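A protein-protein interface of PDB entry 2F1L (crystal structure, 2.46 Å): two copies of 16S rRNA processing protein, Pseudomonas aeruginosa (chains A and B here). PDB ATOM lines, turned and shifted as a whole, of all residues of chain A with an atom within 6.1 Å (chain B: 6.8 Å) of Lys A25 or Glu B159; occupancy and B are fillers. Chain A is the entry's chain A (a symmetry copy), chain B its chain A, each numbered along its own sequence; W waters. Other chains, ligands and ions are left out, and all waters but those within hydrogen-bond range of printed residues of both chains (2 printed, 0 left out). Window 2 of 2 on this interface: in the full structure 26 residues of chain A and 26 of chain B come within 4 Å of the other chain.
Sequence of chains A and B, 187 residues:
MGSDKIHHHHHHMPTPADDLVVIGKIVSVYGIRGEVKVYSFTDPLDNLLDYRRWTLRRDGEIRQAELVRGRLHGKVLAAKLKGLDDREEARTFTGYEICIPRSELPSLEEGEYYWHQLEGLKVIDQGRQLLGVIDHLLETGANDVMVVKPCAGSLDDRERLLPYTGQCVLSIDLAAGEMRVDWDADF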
ATOM      1  N   VAL A  22     -14.130  11.188 -23.578  1.00  0.00           N
ATOM      2  CA  VAL A  22     -12.936  10.478 -23.175  1.00  0.00           C
ATOM      3  C   VAL A  22     -11.956  10.451 -24.339  1.00  0.00           C
ATOM      4  O   VAL A  22     -12.221   9.839 -25.402  1.00  0.00           O
ATOM      5  CB  VAL A  22     -13.244   9.001 -22.791  1.00  0.00           C
ATOM      6  CG1 VAL A  22     -11.982   8.310 -22.267  1.00  0.00           C
ATOM      7  CG2 VAL A  22     -14.344   8.915 -21.774  1.00  0.00           C
ATOM      8  N   ILE A  23     -10.799  11.065 -24.151  1.00  0.00           N
ATOM      9  CA  ILE A  23      -9.817  11.133 -25.248  1.00  0.00           C
ATOM     10  C   ILE A  23      -8.717  10.126 -25.152  1.00  0.00           C
ATOM     11  O   ILE A  23      -7.890  10.056 -26.037  1.00  0.00           O
ATOM     12  CB  ILE A  23      -9.191  12.558 -25.387  1.00  0.00           C
ATOM     13  CG1 ILE A  23      -8.497  12.974 -24.080  1.00  0.00           C
ATOM     14  CG2 ILE A  23     -10.284  13.545 -25.823  1.00  0.00           C
ATOM     15  CD1 ILE A  23      -7.799  14.328 -24.149  1.00  0.00           C
ATOM     16  N   GLY A  24      -8.654   9.401 -24.048  1.00  0.00           N
ATOM     17  CA  GLY A  24      -7.571   8.390 -23.832  1.00  0.00           C
ATOM     18  C   GLY A  24      -7.756   7.663 -22.511  1.00  0.00           C
ATOM     19  O   GLY A  24      -8.729   7.908 -21.783  1.00  0.00           O
ATOM     20  N   LYS A  25      -6.835   6.763 -22.175  1.00  0.00           N
ATOM     21  CA  LYS A  25      -6.939   6.054 -20.920  1.00  0.00           C
ATOM     22  C   LYS A  25      -5.589   5.664 -20.403  1.00  0.00           C
ATOM     23  O   LYS A  25      -4.763   5.169 -21.170  1.00  0.00           O
ATOM     24  CB  LYS A  25      -7.774   4.812 -21.115  1.00  0.00           C
ATOM     25  CG  LYS A  25      -7.946   4.026 -19.809  1.00  0.00           C
ATOM     26  CD  LYS A  25      -9.186   3.169 -19.824  1.00  0.00           C
ATOM     27  CE  LYS A  25      -9.512   2.622 -18.442  1.00  0.00           C
ATOM     28  NZ  LYS A  25     -10.736   1.787 -18.494  1.00  0.00           N
ATOM     29  N   ILE A  26      -5.392   5.850 -19.091  1.00  0.00           N
ATOM     30  CA  ILE A  26      -4.157   5.472 -18.406  1.00  0.00           C
ATOM     31  C   ILE A  26      -4.217   4.015 -18.022  1.00  0.00           C
ATOM     32  O   ILE A  26      -5.093   3.588 -17.280  1.00  0.00           O
ATOM     33  CB  ILE A  26      -3.918   6.342 -17.142  1.00  0.00           C
ATOM     34  CG1 ILE A  26      -3.891   7.829 -17.490  1.00  0.00           C
ATOM     35  CG2 ILE A  26      -2.605   6.009 -16.477  1.00  0.00           C
ATOM     36  CD1 ILE A  26      -3.538   8.748 -16.284  1.00  0.00           C
ATOM     37  N   VAL A  27      -3.279   3.224 -18.527  1.00  0.00           N
ATOM     38  CA  VAL A  27      -3.392   1.757 -18.400  1.00  0.00           C
ATOM     39  C   VAL A  27      -2.247   1.067 -17.712  1.00  0.00           C
ATOM     40  O   VAL A  27      -2.351  -0.097 -17.356  1.00  0.00           O
ATOM     41  CB  VAL A  27      -3.553   1.103 -19.767  1.00  0.00           C
ATOM     42  CG1 VAL A  27      -4.870   1.501 -20.370  1.00  0.00           C
ATOM     43  CG2 VAL A  27      -2.386   1.494 -20.700  1.00  0.00           C
ATOM     44  N   LYS A  37       1.640   4.998 -18.959  1.00  0.00           N
ATOM     45  CA  LYS A  37       1.383   4.491 -20.284  1.00  0.00           C
ATOM     46  C   LYS A  37      -0.107   4.717 -20.547  1.00  0.00           C
ATOM     47  O   LYS A  37      -0.953   4.476 -19.699  1.00  0.00           O
ATOM     48  CB  LYS A  37       1.742   3.026 -20.343  1.00  0.00           C
ATOM     49  CG  LYS A  37       1.809   2.426 -21.734  1.00  0.00           C
ATOM     50  CD  LYS A  37       1.470   0.951 -21.681  1.00  0.00           C
ATOM     51  CE  LYS A  37       2.333   0.057 -22.575  1.00  0.00           C
ATOM     52  NZ  LYS A  37       1.569  -1.216 -22.731  1.00  0.00           N
ATOM     53  N   VAL A  38      -0.383   5.215 -21.734  1.00  0.00           N
ATOM     54  CA  VAL A  38      -1.649   5.820 -22.076  1.00  0.00           C
ATOM     55  C   VAL A  38      -2.035   5.350 -23.469  1.00  0.00           C
ATOM     56  O   VAL A  38      -1.218   5.381 -24.385  1.00  0.00           O
ATOM     57  CB  VAL A  38      -1.509   7.363 -22.043  1.00  0.00           C
ATOM     58  CG1 VAL A  38      -2.623   8.035 -22.768  1.00  0.00           C
ATOM     59  CG2 VAL A  38      -1.498   7.844 -20.593  1.00  0.00           C
ATOM     60  N   TYR A  39      -3.262   4.867 -23.619  1.00  0.00           N
ATOM     61  CA  TYR A  39      -3.797   4.674 -24.937  1.00  0.00           C
ATOM     62  C   TYR A  39      -4.455   6.005 -25.338  1.00  0.00           C
ATOM     63  O   TYR A  39      -5.071   6.684 -24.496  1.00  0.00           O
ATOM     64  CB  TYR A  39      -4.819   3.531 -24.969  1.00  0.00           C
ATOM     65  CG  TYR A  39      -4.285   2.114 -24.801  1.00  0.00           C
ATOM     66  CD1 TYR A  39      -3.112   1.709 -25.384  1.00  0.00           C
ATOM     67  CD2 TYR A  39      -5.033   1.154 -24.126  1.00  0.00           C
ATOM     68  CE1 TYR A  39      -2.667   0.387 -25.271  1.00  0.00           C
ATOM     69  CE2 TYR A  39      -4.603  -0.155 -24.008  1.00  0.00           C
ATOM     70  CZ  TYR A  39      -3.409  -0.533 -24.575  1.00  0.00           C
ATOM     71  OH  TYR A  39      -2.948  -1.833 -24.447  1.00  0.00           O
ATOM     72  N   SER A  40      -4.311   6.399 -26.602  1.00  0.00           N
ATOM     73  CA  SER A  40      -4.941   7.635 -27.078  1.00  0.00           C
ATOM     74  C   SER A  40      -6.107   7.350 -27.998  1.00  0.00           C
ATOM     75  O   SER A  40      -6.000   6.489 -28.833  1.00  0.00           O
ATOM     76  CB  SER A  40      -3.942   8.476 -27.841  1.00  0.00           C
ATOM     77  OG  SER A  40      -4.607   9.488 -28.555  1.00  0.00           O
ATOM     78  N   PHE A  41      -7.187   8.104 -27.871  1.00  0.00           N
ATOM     79  CA  PHE A  41      -8.376   7.939 -28.716  1.00  0.00           C
ATOM     80  C   PHE A  41      -8.581   9.096 -29.708  1.00  0.00           C
ATOM     81  O   PHE A  41      -9.664   9.236 -30.368  1.00  0.00           O
ATOM     82  CB  PHE A  41      -9.623   7.778 -27.812  1.00  0.00           C
ATOM     83  CG  PHE A  41      -9.498   6.675 -26.781  1.00  0.00           C
ATOM     84  CD1 PHE A  41      -8.842   5.485 -27.087  1.00  0.00           C
ATOM     85  CD2 PHE A  41     -10.082   6.806 -25.529  1.00  0.00           C
ATOM     86  CE1 PHE A  41      -8.705   4.480 -26.136  1.00  0.00           C
ATOM     87  CE2 PHE A  41      -9.951   5.803 -24.558  1.00  0.00           C
ATOM     88  CZ  PHE A  41      -9.274   4.639 -24.869  1.00  0.00           C
ATOM     89  N   LEU A  48      -3.718  13.869 -28.391  1.00  0.00           N
ATOM     90  CA  LEU A  48      -3.850  13.816 -26.948  1.00  0.00           C
ATOM     91  C   LEU A  48      -2.829  14.698 -26.216  1.00  0.00           C
ATOM     92  O   LEU A  48      -3.148  15.292 -25.204  1.00  0.00           O
ATOM     93  CB  LEU A  48      -3.721  12.365 -26.489  1.00  0.00           C
ATOM     94  CG  LEU A  48      -3.786  12.101 -24.982  1.00  0.00           C
ATOM     95  CD1 LEU A  48      -5.076  12.607 -24.459  1.00  0.00           C
ATOM     96  CD2 LEU A  48      -3.704  10.674 -24.689  1.00  0.00           C
ATOM     97  N   GLY A  95      -6.137   2.808 -14.892  1.00  0.00           N
ATOM     98  CA  GLY A  95      -7.587   2.676 -14.960  1.00  0.00           C
ATOM     99  C   GLY A  95      -8.324   3.999 -15.026  1.00  0.00           C
ATOM    100  O   GLY A  95      -9.537   4.001 -15.114  1.00  0.00           O
ATOM    101  N   TYR A  96      -7.613   5.125 -14.988  1.00  0.00           N
ATOM    102  CA  TYR A  96      -8.245   6.442 -15.151  1.00  0.00           C
ATOM    103  C   TYR A  96      -8.462   6.775 -16.610  1.00  0.00           C
ATOM    104  O   TYR A  96      -7.540   6.753 -17.422  1.00  0.00           O
ATOM    105  CB  TYR A  96      -7.370   7.546 -14.580  1.00  0.00           C
ATOM    106  CG  TYR A  96      -7.569   7.794 -13.106  1.00  0.00           C
ATOM    107  CD1 TYR A  96      -8.789   8.190 -12.611  1.00  0.00           C
ATOM    108  CD2 TYR A  96      -6.524   7.682 -12.216  1.00  0.00           C
ATOM    109  CE1 TYR A  96      -8.972   8.430 -11.268  1.00  0.00           C
ATOM    110  CE2 TYR A  96      -6.709   7.919 -10.869  1.00  0.00           C
ATOM    111  CZ  TYR A  96      -7.927   8.288 -10.412  1.00  0.00           C
ATOM    112  OH  TYR A  96      -8.106   8.521  -9.083  1.00  0.00           O
ATOM    113  N   GLU A  97      -9.696   7.089 -16.952  1.00  0.00           N
ATOM    114  CA  GLU A  97      -9.994   7.649 -18.250  1.00  0.00           C
ATOM    115  C   GLU A  97      -9.499   9.069 -18.257  1.00  0.00           C
ATOM    116  O   GLU A  97      -9.637   9.785 -17.260  1.00  0.00           O
ATOM    117  CB  GLU A  97     -11.487   7.653 -18.484  1.00  0.00           C
ATOM    118  CG  GLU A  97     -12.067   6.265 -18.569  1.00  0.00           C
ATOM    119  CD  GLU A  97     -13.569   6.260 -18.688  1.00  0.00           C
ATOM    120  OE1 GLU A  97     -14.214   7.270 -18.272  1.00  0.00           O
ATOM    121  OE2 GLU A  97     -14.094   5.229 -19.188  1.00  0.00           O
ATOM    122  N   ILE A  98      -8.915   9.478 -19.374  1.00  0.00           N
ATOM    123  CA  ILE A  98      -8.461  10.856 -19.545  1.00  0.00           C
ATOM    124  C   ILE A  98      -9.575  11.581 -20.264  1.00  0.00           C
ATOM    125  O   ILE A  98      -9.862  11.233 -21.404  1.00  0.00           O
ATOM    126  CB  ILE A  98      -7.211  10.935 -20.429  1.00  0.00           C
ATOM    127  CG1 ILE A  98      -6.082  10.070 -19.856  1.00  0.00           C
ATOM    128  CG2 ILE A  98      -6.789  12.420 -20.592  1.00  0.00           C
ATOM    129  CD1 ILE A  98      -5.024   9.707 -20.812  1.00  0.00           C
ATOM    130  N   LEU B 131     -11.512 -12.336 -27.190  1.00  0.00           N
ATOM    131  CA  LEU B 131     -10.962 -11.268 -26.365  1.00  0.00           C
ATOM    132  C   LEU B 131     -11.890 -10.887 -25.240  1.00  0.00           C
ATOM    133  O   LEU B 131     -11.462 -10.303 -24.264  1.00  0.00           O
ATOM    134  CB  LEU B 131     -10.745 -10.029 -27.211  1.00  0.00           C
ATOM    135  CG  LEU B 131      -9.960 -10.189 -28.518  1.00  0.00           C
ATOM    136  CD1 LEU B 131      -9.705  -8.820 -29.180  1.00  0.00           C
ATOM    137  CD2 LEU B 131      -8.639 -10.901 -28.279  1.00  0.00           C
ATOM    138  N   HIS B 136     -19.380  -1.768 -22.849  1.00  0.00           N
ATOM    139  CA  HIS B 136     -20.021  -0.505 -23.237  1.00  0.00           C
ATOM    140  C   HIS B 136     -19.123   0.225 -24.215  1.00  0.00           C
ATOM    141  O   HIS B 136     -18.052  -0.285 -24.574  1.00  0.00           O
ATOM    142  CB  HIS B 136     -20.405   0.395 -22.047  1.00  0.00           C
ATOM    143  CG  HIS B 136     -19.250   0.866 -21.215  1.00  0.00           C
ATOM    144  ND1 HIS B 136     -18.634   0.065 -20.271  1.00  0.00           N
ATOM    145  CD2 HIS B 136     -18.650   2.084 -21.122  1.00  0.00           C
ATOM    146  CE1 HIS B 136     -17.684   0.758 -19.654  1.00  0.00           C
ATOM    147  NE2 HIS B 136     -17.665   1.985 -20.157  1.00  0.00           N
ATOM    148  N   LEU B 138     -17.635   4.154 -25.714  1.00  0.00           N
ATOM    149  CA  LEU B 138     -17.253   5.492 -25.280  1.00  0.00           C
ATOM    150  C   LEU B 138     -17.300   6.446 -26.444  1.00  0.00           C
ATOM    151  O   LEU B 138     -16.901   6.120 -27.539  1.00  0.00           O
ATOM    152  CB  LEU B 138     -15.835   5.526 -24.713  1.00  0.00           C
ATOM    153  CG  LEU B 138     -15.486   4.633 -23.525  1.00  0.00           C
ATOM    154  CD1 LEU B 138     -13.999   4.816 -23.198  1.00  0.00           C
ATOM    155  CD2 LEU B 138     -16.320   4.888 -22.279  1.00  0.00           C
ATOM    156  N   VAL B 147     -15.318  -0.796 -25.064  1.00  0.00           N
ATOM    157  CA  VAL B 147     -14.675  -1.327 -23.867  1.00  0.00           C
ATOM    158  C   VAL B 147     -14.980  -2.814 -23.844  1.00  0.00           C
ATOM    159  O   VAL B 147     -16.136  -3.214 -23.673  1.00  0.00           O
ATOM    160  CB  VAL B 147     -15.182  -0.630 -22.550  1.00  0.00           C
ATOM    161  CG1 VAL B 147     -14.414  -1.124 -21.341  1.00  0.00           C
ATOM    162  CG2 VAL B 147     -15.013   0.849 -22.640  1.00  0.00           C
ATOM    163  N   VAL B 148     -13.932  -3.616 -24.046  1.00  0.00           N
ATOM    164  CA  VAL B 148     -14.020  -5.087 -24.073  1.00  0.00           C
ATOM    165  C   VAL B 148     -13.553  -5.682 -22.745  1.00  0.00           C
ATOM    166  O   VAL B 148     -12.394  -5.504 -22.353  1.00  0.00           O
ATOM    167  CB  VAL B 148     -13.192  -5.613 -25.216  1.00  0.00           C
ATOM    168  CG1 VAL B 148     -13.288  -7.125 -25.265  1.00  0.00           C
ATOM    169  CG2 VAL B 148     -13.730  -5.010 -26.541  1.00  0.00           C
ATOM    170  N   LYS B 149     -14.474  -6.318 -22.017  1.00  0.00           N
ATOM    171  CA  LYS B 149     -14.183  -6.860 -20.669  1.00  0.00           C
ATOM    172  C   LYS B 149     -13.892  -8.338 -20.863  1.00  0.00           C
ATOM    173  O   LYS B 149     -14.518  -8.984 -21.689  1.00  0.00           O
ATOM    174  CB  LYS B 149     -15.358  -6.664 -19.684  1.00  0.00           C
ATOM    175  N   PRO B 150     -12.960  -8.887 -20.095  1.00  0.00           N
ATOM    176  CA  PRO B 150     -12.738 -10.332 -20.160  1.00  0.00           C
ATOM    177  C   PRO B 150     -13.907 -11.064 -19.504  1.00  0.00           C
ATOM    178  O   PRO B 150     -14.580 -10.494 -18.643  1.00  0.00           O
ATOM    179  CB  PRO B 150     -11.488 -10.540 -19.300  1.00  0.00           C
ATOM    180  CG  PRO B 150     -11.608  -9.477 -18.265  1.00  0.00           C
ATOM    181  CD  PRO B 150     -12.145  -8.251 -19.047  1.00  0.00           C
ATOM    182  N   ASP B 156      -7.621 -13.945 -21.799  1.00  0.00           N
ATOM    183  CA  ASP B 156      -6.893 -13.556 -20.590  1.00  0.00           C
ATOM    184  C   ASP B 156      -7.756 -12.715 -19.646  1.00  0.00           C
ATOM    185  O   ASP B 156      -8.958 -12.901 -19.605  1.00  0.00           O
ATOM    186  CB  ASP B 156      -5.576 -12.863 -20.969  1.00  0.00           C
ATOM    187  CG  ASP B 156      -5.775 -11.611 -21.824  1.00  0.00           C
ATOM    188  OD1 ASP B 156      -6.846 -10.952 -21.750  1.00  0.00           O
ATOM    189  OD2 ASP B 156      -4.823 -11.275 -22.560  1.00  0.00           O
ATOM    190  N   ASP B 157      -7.125 -11.810 -18.900  1.00  0.00           N
ATOM    191  CA  ASP B 157      -7.739 -11.045 -17.817  1.00  0.00           C
ATOM    192  C   ASP B 157      -7.832  -9.588 -18.137  1.00  0.00           C
ATOM    193  O   ASP B 157      -8.256  -8.796 -17.276  1.00  0.00           O
ATOM    194  CB  ASP B 157      -6.882 -11.174 -16.553  1.00  0.00           C
ATOM    195  CG  ASP B 157      -7.224 -12.394 -15.758  1.00  0.00           C
ATOM    196  OD1 ASP B 157      -8.116 -13.136 -16.226  1.00  0.00           O
ATOM    197  OD2 ASP B 157      -6.622 -12.607 -14.674  1.00  0.00           O
ATOM    198  N   ARG B 158      -7.444  -9.233 -19.364  1.00  0.00           N
ATOM    199  CA  ARG B 158      -7.195  -7.853 -19.717  1.00  0.00           C
ATOM    200  C   ARG B 158      -8.406  -7.225 -20.328  1.00  0.00           C
ATOM    201  O   ARG B 158      -8.997  -7.795 -21.253  1.00  0.00           O
ATOM    202  CB  ARG B 158      -6.089  -7.750 -20.770  1.00  0.00           C
ATOM    203  CG  ARG B 158      -4.684  -8.040 -20.290  1.00  0.00           C
ATOM    204  CD  ARG B 158      -3.689  -7.739 -21.407  1.00  0.00           C
ATOM    205  NE  ARG B 158      -3.732  -6.312 -21.722  1.00  0.00           N
ATOM    206  CZ  ARG B 158      -3.648  -5.788 -22.935  1.00  0.00           C
ATOM    207  NH1 ARG B 158      -3.521  -6.539 -24.016  1.00  0.00           N
ATOM    208  NH2 ARG B 158      -3.726  -4.484 -23.061  1.00  0.00           N
ATOM    209  N   GLU B 159      -8.719  -6.016 -19.871  1.00  0.00           N
ATOM    210  CA  GLU B 159      -9.679  -5.165 -20.561  1.00  0.00           C
ATOM    211  C   GLU B 159      -8.978  -4.568 -21.778  1.00  0.00           C
ATOM    212  O   GLU B 159      -7.783  -4.289 -21.743  1.00  0.00           O
ATOM    213  CB  GLU B 159     -10.234  -4.072 -19.637  1.00  0.00           C
ATOM    214  CG  GLU B 159     -10.778  -2.847 -20.343  1.00  0.00           C
ATOM    215  CD  GLU B 159     -11.114  -1.729 -19.379  1.00  0.00           C
ATOM    216  OE1 GLU B 159     -11.994  -1.949 -18.538  1.00  0.00           O
ATOM    217  OE2 GLU B 159     -10.507  -0.629 -19.472  1.00  0.00           O
ATOM    218  N   ARG B 160      -9.723  -4.380 -22.860  1.00  0.00           N
ATOM    219  CA  ARG B 160      -9.165  -3.781 -24.042  1.00  0.00           C
ATOM    220  C   ARG B 160     -10.052  -2.694 -24.602  1.00  0.00           C
ATOM    221  O   ARG B 160     -11.236  -2.647 -24.344  1.00  0.00           O
ATOM    222  CB  ARG B 160      -8.934  -4.852 -25.100  1.00  0.00           C
ATOM    223  CG  ARG B 160      -7.782  -5.766 -24.797  1.00  0.00           C
ATOM    224  CD  ARG B 160      -7.685  -6.802 -25.861  1.00  0.00           C
ATOM    225  NE  ARG B 160      -6.530  -7.683 -25.699  1.00  0.00           N
ATOM    226  CZ  ARG B 160      -6.513  -8.701 -24.860  1.00  0.00           C
ATOM    227  NH1 ARG B 160      -7.567  -8.942 -24.087  1.00  0.00           N
ATOM    228  NH2 ARG B 160      -5.448  -9.469 -24.775  1.00  0.00           N
ATOM    229  N   LEU B 161      -9.470  -1.818 -25.396  1.00  0.00           N
ATOM    230  CA  LEU B 161     -10.217  -0.685 -25.902  1.00  0.00           C
ATOM    231  C   LEU B 161     -10.003  -0.567 -27.401  1.00  0.00           C
ATOM    232  O   LEU B 161      -8.915  -0.169 -27.871  1.00  0.00           O
ATOM    233  CB  LEU B 161      -9.756   0.565 -25.182  1.00  0.00           C
ATOM    234  CG  LEU B 161     -10.033   0.467 -23.695  1.00  0.00           C
ATOM    235  CD1 LEU B 161      -8.875   1.078 -22.935  1.00  0.00           C
ATOM    236  CD2 LEU B 161     -11.359   1.119 -23.342  1.00  0.00           C
ATOM    237  N   PHE B 187      -1.421  -5.956 -28.054  1.00  0.00           N
ATOM    238  CA  PHE B 187      -1.393  -4.505 -27.966  1.00  0.00           C
ATOM    239  C   PHE B 187      -1.963  -3.966 -26.656  1.00  0.00           C
ATOM    240  O   PHE B 187      -3.033  -4.358 -26.172  1.00  0.00           O
ATOM    241  CB  PHE B 187      -2.097  -3.829 -29.141  1.00  0.00           C
ATOM    242  CG  PHE B 187      -2.004  -2.344 -29.081  1.00  0.00           C
ATOM    243  CD1 PHE B 187      -0.761  -1.723 -29.182  1.00  0.00           C
ATOM    244  CD2 PHE B 187      -3.127  -1.573 -28.819  1.00  0.00           C
ATOM    245  CE1 PHE B 187      -0.653  -0.367 -29.067  1.00  0.00           C
ATOM    246  CE2 PHE B 187      -3.025  -0.198 -28.703  1.00  0.00           C
ATOM    247  CZ  PHE B 187      -1.790   0.409 -28.830  1.00  0.00           C
ATOM    248  OXT PHE B 187      -1.326  -3.075 -26.082  1.00  0.00           O
HETATM  249  O   HOH W   1     -16.561   4.180 -18.961  1.00  0.00           O
HETATM  250  O   HOH W   2       1.241  -1.828 -25.749  1.00  0.00           O
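No position is printed for both chains. Of the 5 pairs that touch across the chains among the printed residues, none has its exchanged pair printed and touching as well.
Among the printed residues, merely in contact across the chains: Lys A25 with Leu B161 (3.8 Å) and Glu A97 with Leu B138 (3.8 Å).
Of the 14 printed residues of chain B, 5 touch a printed residue of chain A. Hydrophobic or aromatic side chains of chain B that line the printed part of chain A: Leu B138, Leu B161 and Phe B187. Along chain B the printed residues that touch a printed residue of chain A span positions 138 to 187. Of the 16 printed residues of chain A, 3 touch a printed residue of chain B. Hydrophobic or aromatic side chains of chain A within 4 Å of the printed part of chain B: Tyr A39.
Lys A25 touches just these residues of chain B: Glu B159 (2.6 Å) and Leu B161 (3.8 Å). Val A38 touches none of the printed residues of chain B. Of chain A, only Lys A25 comes within 4 Å of Glu B159. Of the printed residues of chain A, Leu B161 touches Lys A25 (3.8 Å). Of the printed residues of chain A, Phe B187 touches Tyr A39 (2.6 Å). The nearest printed residue of chain A that does not touch Arg B158 is Lys A37 (6.2 Å).
NH2 of Arg B158 sits at hydrogen-bond distance from OH of Tyr A39 (3.1 Å). OH of Tyr A39 is in hydrogen-bond range of OXT of Phe B187, at 2.6 Å. The side-chain amino group of Lys A25 lies within salt-bridge range of the side-chain carboxylate of Glu B159, 2.6 Å away.
Water W1 lies within hydrogen-bond range of the side-chain carboxylate of Glu A97 and a ring nitrogen (NE2) of His B136. Water W2 lies within hydrogen-bond range of the chain-end carboxylate of Phe B187 and the side-chain amino group of Lys A37.
NH1 of Arg B160 sits at hydrogen-bond distance from O of Arg B158 (3.4 Å). NH1 of Arg B158 lies within salt-bridge range of O of Phe B187, 3.1 Å away. The backbone NH (N) of Arg B158 sits at hydrogen-bond distance from the side-chain carboxylate (OD1) of Asp B156. The backbone NH of Tyr A39 is in hydrogen-bond range of the backbone carbonyl oxygen of Lys A25, at 2.9 Å.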
